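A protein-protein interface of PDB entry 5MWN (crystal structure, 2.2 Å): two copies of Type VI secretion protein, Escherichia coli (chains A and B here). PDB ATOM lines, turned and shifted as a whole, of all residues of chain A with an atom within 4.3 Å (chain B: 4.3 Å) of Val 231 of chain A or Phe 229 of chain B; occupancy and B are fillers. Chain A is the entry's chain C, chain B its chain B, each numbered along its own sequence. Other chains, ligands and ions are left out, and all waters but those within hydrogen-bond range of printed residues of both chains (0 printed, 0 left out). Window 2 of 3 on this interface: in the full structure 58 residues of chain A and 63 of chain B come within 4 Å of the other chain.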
ATOM      1  N   PHE A 229     -24.837  -4.635  25.368  1.00  0.00           N
ATOM      2  CA  PHE A 229     -25.446  -3.878  24.272  1.00  0.00           C
ATOM      3  C   PHE A 229     -25.242  -2.377  24.469  1.00  0.00           C
ATOM      4  O   PHE A 229     -25.380  -1.609  23.510  1.00  0.00           O
ATOM      5  CB  PHE A 229     -26.955  -4.194  24.148  1.00  0.00           C
ATOM      6  CG  PHE A 229     -27.298  -5.569  23.616  1.00  0.00           C
ATOM      7  CD1 PHE A 229     -27.997  -6.480  24.397  1.00  0.00           C
ATOM      8  CD2 PHE A 229     -26.950  -5.940  22.322  1.00  0.00           C
ATOM      9  CE1 PHE A 229     -28.314  -7.750  23.904  1.00  0.00           C
ATOM     10  CE2 PHE A 229     -27.257  -7.213  21.834  1.00  0.00           C
ATOM     11  CZ  PHE A 229     -27.942  -8.107  22.626  1.00  0.00           C
ATOM     12  N   ALA A 230     -24.912  -1.956  25.711  1.00  0.00           N
ATOM     13  CA  ALA A 230     -24.773  -0.549  26.056  1.00  0.00           C
ATOM     14  C   ALA A 230     -23.496   0.065  25.535  1.00  0.00           C
ATOM     15  O   ALA A 230     -22.446  -0.559  25.631  1.00  0.00           O
ATOM     16  CB  ALA A 230     -24.854  -0.358  27.551  1.00  0.00           C
ATOM     17  N   VAL A 231     -23.601   1.290  24.982  1.00  0.00           N
ATOM     18  CA  VAL A 231     -22.500   2.068  24.409  1.00  0.00           C
ATOM     19  C   VAL A 231     -21.443   2.424  25.456  1.00  0.00           C
ATOM     20  O   VAL A 231     -20.266   2.477  25.113  1.00  0.00           O
ATOM     21  CB  VAL A 231     -22.992   3.322  23.643  1.00  0.00           C
ATOM     22  N   ALA A 232     -21.847   2.663  26.719  1.00  0.00           N
ATOM     23  CA  ALA A 232     -20.955   2.997  27.843  1.00  0.00           C
ATOM     24  C   ALA A 232     -20.131   1.787  28.310  1.00  0.00           C
ATOM     25  O   ALA A 232     -18.999   1.957  28.768  1.00  0.00           O
ATOM     26  CB  ALA A 232     -21.768   3.538  29.005  1.00  0.00           C
ATOM     27  N   ASP A 233     -20.730   0.571  28.228  1.00  0.00           N
ATOM     28  CA  ASP A 233     -20.132  -0.718  28.606  1.00  0.00           C
ATOM     29  C   ASP A 233     -18.925  -1.047  27.730  1.00  0.00           C
ATOM     30  O   ASP A 233     -18.035  -1.773  28.171  1.00  0.00           O
ATOM     31  CB  ASP A 233     -21.173  -1.851  28.533  1.00  0.00           C
ATOM     32  N   VAL A 234     -18.895  -0.487  26.506  1.00  0.00           N
ATOM     33  CA  VAL A 234     -17.843  -0.626  25.500  1.00  0.00           C
ATOM     34  C   VAL A 234     -16.489  -0.089  26.036  1.00  0.00           C
ATOM     35  O   VAL A 234     -15.521  -0.841  26.054  1.00  0.00           O
ATOM     36  CB  VAL A 234     -18.305   0.007  24.156  1.00  0.00           C
ATOM     37  CG1 VAL A 234     -17.145   0.344  23.239  1.00  0.00           C
ATOM     38  CG2 VAL A 234     -19.309  -0.893  23.444  1.00  0.00           C
ATOM     39  N   SER A 235     -16.445   1.175  26.514  1.00  0.00           N
ATOM     40  CA  SER A 235     -15.262   1.804  27.112  1.00  0.00           C
ATOM     41  C   SER A 235     -14.917   1.151  28.450  1.00  0.00           C
ATOM     42  O   SER A 235     -13.739   1.058  28.796  1.00  0.00           O
ATOM     43  CB  SER A 235     -15.496   3.296  27.328  1.00  0.00           C
ATOM     44  OG  SER A 235     -15.754   3.960  26.102  1.00  0.00           O
ATOM     45  N   TRP A 238     -13.292  -2.329  27.922  1.00  0.00           N
ATOM     46  CA  TRP A 238     -11.992  -2.065  27.311  1.00  0.00           C
ATOM     47  C   TRP A 238     -10.949  -1.535  28.318  1.00  0.00           C
ATOM     48  O   TRP A 238      -9.778  -1.906  28.220  1.00  0.00           O
ATOM     49  CB  TRP A 238     -12.164  -1.158  26.086  1.00  0.00           C
ATOM     50  CG  TRP A 238     -12.807  -1.855  24.909  1.00  0.00           C
ATOM     51  CD1 TRP A 238     -13.021  -3.198  24.762  1.00  0.00           C
ATOM     52  CD2 TRP A 238     -13.320  -1.237  23.720  1.00  0.00           C
ATOM     53  NE1 TRP A 238     -13.635  -3.454  23.558  1.00  0.00           N
ATOM     54  CE2 TRP A 238     -13.819  -2.269  22.892  1.00  0.00           C
ATOM     55  CE3 TRP A 238     -13.418   0.093  23.277  1.00  0.00           C
ATOM     56  CZ2 TRP A 238     -14.387  -2.013  21.637  1.00  0.00           C
ATOM     57  CZ3 TRP A 238     -13.954   0.341  22.021  1.00  0.00           C
ATOM     58  CH2 TRP A 238     -14.431  -0.702  21.217  1.00  0.00           C
ATOM     59  N   THR A 277      -5.092   5.903  26.000  1.00  0.00           N
ATOM     60  CA  THR A 277      -6.046   5.781  24.880  1.00  0.00           C
ATOM     61  C   THR A 277      -7.411   6.442  25.224  1.00  0.00           C
ATOM     62  O   THR A 277      -8.118   6.920  24.332  1.00  0.00           O
ATOM     63  CB  THR A 277      -6.251   4.282  24.508  1.00  0.00           C
ATOM     64  OG1 THR A 277      -5.011   3.630  24.203  1.00  0.00           O
ATOM     65  CG2 THR A 277      -7.199   4.078  23.343  1.00  0.00           C
ATOM     66  N   ARG B 219     -10.166  10.515  17.608  1.00  0.00           N
ATOM     67  CA  ARG B 219     -11.188  10.111  18.582  1.00  0.00           C
ATOM     68  C   ARG B 219     -12.137  11.265  18.822  1.00  0.00           C
ATOM     69  O   ARG B 219     -11.702  12.411  18.949  1.00  0.00           O
ATOM     70  CB  ARG B 219     -10.616   9.682  19.947  1.00  0.00           C
ATOM     71  CG  ARG B 219      -9.363   8.851  19.921  1.00  0.00           C
ATOM     72  CD  ARG B 219      -8.263   9.681  20.510  1.00  0.00           C
ATOM     73  NE  ARG B 219      -7.916   9.290  21.861  1.00  0.00           N
ATOM     74  CZ  ARG B 219      -7.220  10.031  22.715  1.00  0.00           C
ATOM     75  NH1 ARG B 219      -6.934   9.583  23.918  1.00  0.00           N
ATOM     76  NH2 ARG B 219      -6.787  11.236  22.345  1.00  0.00           N
ATOM     77  N   ALA B 227     -12.281  10.344  26.106  1.00  0.00           N
ATOM     78  CA  ALA B 227     -12.513   9.878  24.743  1.00  0.00           C
ATOM     79  C   ALA B 227     -13.800   9.064  24.671  1.00  0.00           C
ATOM     80  O   ALA B 227     -14.125   8.338  25.614  1.00  0.00           O
ATOM     81  CB  ALA B 227     -11.339   9.032  24.278  1.00  0.00           C
ATOM     82  N   ASP B 228     -14.528   9.181  23.546  1.00  0.00           N
ATOM     83  CA  ASP B 228     -15.774   8.457  23.319  1.00  0.00           C
ATOM     84  C   ASP B 228     -15.527   7.212  22.483  1.00  0.00           C
ATOM     85  O   ASP B 228     -14.982   7.305  21.384  1.00  0.00           O
ATOM     86  CB  ASP B 228     -16.814   9.360  22.631  1.00  0.00           C
ATOM     87  CG  ASP B 228     -18.253   8.994  22.944  1.00  0.00           C
ATOM     88  OD1 ASP B 228     -18.589   8.880  24.143  1.00  0.00           O
ATOM     89  OD2 ASP B 228     -19.054   8.876  21.993  1.00  0.00           O
ATOM     90  N   PHE B 229     -15.912   6.043  23.012  1.00  0.00           N
ATOM     91  CA  PHE B 229     -15.761   4.776  22.310  1.00  0.00           C
ATOM     92  C   PHE B 229     -17.079   4.017  22.221  1.00  0.00           C
ATOM     93  O   PHE B 229     -17.666   3.645  23.240  1.00  0.00           O
ATOM     94  CB  PHE B 229     -14.620   3.918  22.888  1.00  0.00           C
ATOM     95  CG  PHE B 229     -13.235   4.492  22.667  1.00  0.00           C
ATOM     96  CD1 PHE B 229     -12.684   4.555  21.392  1.00  0.00           C
ATOM     97  CD2 PHE B 229     -12.471   4.938  23.738  1.00  0.00           C
ATOM     98  CE1 PHE B 229     -11.409   5.078  21.189  1.00  0.00           C
ATOM     99  CE2 PHE B 229     -11.190   5.454  23.538  1.00  0.00           C
ATOM    100  CZ  PHE B 229     -10.669   5.527  22.262  1.00  0.00           C
ATOM    101  N   ALA B 230     -17.547   3.829  20.979  1.00  0.00           N
ATOM    102  CA  ALA B 230     -18.780   3.154  20.575  1.00  0.00           C
ATOM    103  C   ALA B 230     -18.462   1.852  19.786  1.00  0.00           C
ATOM    104  O   ALA B 230     -17.289   1.476  19.658  1.00  0.00           O
ATOM    105  CB  ALA B 230     -19.623   4.114  19.730  1.00  0.00           C
ATOM    106  N   ASP B 233     -16.119   2.277  16.698  1.00  0.00           N
ATOM    107  CA  ASP B 233     -14.708   2.491  17.025  1.00  0.00           C
ATOM    108  C   ASP B 233     -13.967   1.219  17.476  1.00  0.00           C
ATOM    109  O   ASP B 233     -12.882   1.334  18.056  1.00  0.00           O
ATOM    110  CB  ASP B 233     -14.561   3.601  18.084  1.00  0.00           C
ATOM    111  CG  ASP B 233     -15.351   4.861  17.812  1.00  0.00           C
ATOM    112  OD1 ASP B 233     -16.246   5.183  18.623  1.00  0.00           O
ATOM    113  OD2 ASP B 233     -15.058   5.541  16.804  1.00  0.00           O
ATOM    114  N   LEU B 236     -10.698   1.473  15.810  1.00  0.00           N
ATOM    115  CA  LEU B 236      -9.993   2.656  16.316  1.00  0.00           C
ATOM    116  C   LEU B 236      -9.407   2.458  17.722  1.00  0.00           C
ATOM    117  O   LEU B 236      -8.243   2.809  17.930  1.00  0.00           O
ATOM    118  CB  LEU B 236     -10.888   3.917  16.246  1.00  0.00           C
ATOM    119  CG  LEU B 236     -10.258   5.338  16.377  1.00  0.00           C
ATOM    120  CD1 LEU B 236     -10.356   5.876  17.779  1.00  0.00           C
ATOM    121  CD2 LEU B 236      -8.841   5.437  15.813  1.00  0.00           C
ATOM    122  N   PHE B 237     -10.191   1.898  18.671  1.00  0.00           N
ATOM    123  CA  PHE B 237      -9.693   1.661  20.022  1.00  0.00           C
ATOM    124  C   PHE B 237      -8.567   0.647  20.047  1.00  0.00           C
ATOM    125  O   PHE B 237      -7.514   0.967  20.589  1.00  0.00           O
ATOM    126  CB  PHE B 237     -10.795   1.234  21.014  1.00  0.00           C
ATOM    127  CG  PHE B 237     -10.222   0.627  22.283  1.00  0.00           C
ATOM    128  CD1 PHE B 237      -9.702   1.436  23.288  1.00  0.00           C
ATOM    129  CD2 PHE B 237     -10.138  -0.755  22.441  1.00  0.00           C
ATOM    130  CE1 PHE B 237      -9.113   0.876  24.426  1.00  0.00           C
ATOM    131  CE2 PHE B 237      -9.556  -1.312  23.585  1.00  0.00           C
ATOM    132  CZ  PHE B 237      -9.048  -0.492  24.568  1.00  0.00           C
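The backbone carbonyl oxygen (O) of Val 231 of chain A lies close to the backbone carbonyl oxygen (O) of Phe 229 of chain B, at 3.4 Å.
OG of Ser 235 of chain A lies close to O of Phe 229 of chain B.
The guanidinium group (NH1) of Arg 219 of chain B is in hydrogen-bond range of the backbone carbonyl oxygen (O) of Thr 277 of chain A.
The backbone NH of Ala 230 of chain B lies within hydrogen-bond range of the side-chain carboxylate of Asp 233 of chain B (3.0 Å).
Val 234 of chain A touches Phe 229 of chain B.
Ala 230 of chain B touches Val 234 of chain A.
CB of Phe 229 of chain B touches CZ3 of Trp 238 of chain A, 3.7 Å away.
CH2 of Trp 238 of chain A touches O of Ala 230 of chain B (3.9 Å).
Trp 238 of chain A touches Phe 237 of chain B (CE3 to CG, 3.4 Å).
Thr 277 of chain A touches Ala 227 of chain B.
Thr 277 of chain A touches Phe 229 of chain B (O to CE2, 3.5 Å).
Thr 277 of chain A touches Phe 237 of chain B (CG2 to CD1, 3.6 Å).
Of the printed residues of chain B, Val 231 of chain A touches Phe 229 (3.4 Å).
Phe 229 of chain B touches just these residues of chain A: Val 231, Val 234, Ser 235, Trp 238 and Thr 277.
Printed residues of chain B within 4 Å of Val 234 of chain A: Phe 229 (3.3 Å) and Ala 230 (3.8 Å).
Printed residues of chain B within 4 Å of Ser 235 of chain A: Phe 229 (3.4 Å).
Printed residues of chain A within 4 Å of Phe 237 of chain B: Trp 238 (3.4 Å) and Thr 277 (3.6 Å).
Leu 236 of chain B touches none of the printed residues of chain A.
The nearest printed residue of chain B that does not touch Val 231 of chain A is Ala 230 of chain B (4.8 Å).
Hydrophobic or aromatic side chains of chain A within 4 Å of the printed part of chain B: Val 234 and Trp 238.
Of the 8 printed residues of chain B, 5 touch a printed residue of chain A.
Hydrophobic or aromatic side chains of chain B within 4 Å of the printed part of chain A: Ala 227, Phe 229 and Phe 237.
Among the printed residues, 11 pairs touch across the chains.
Positions printed for both chains: 229, 230 and 233.
Of the 11 pairs that touch across the chains among the printed residues, none has its exchanged pair printed and touching as well.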
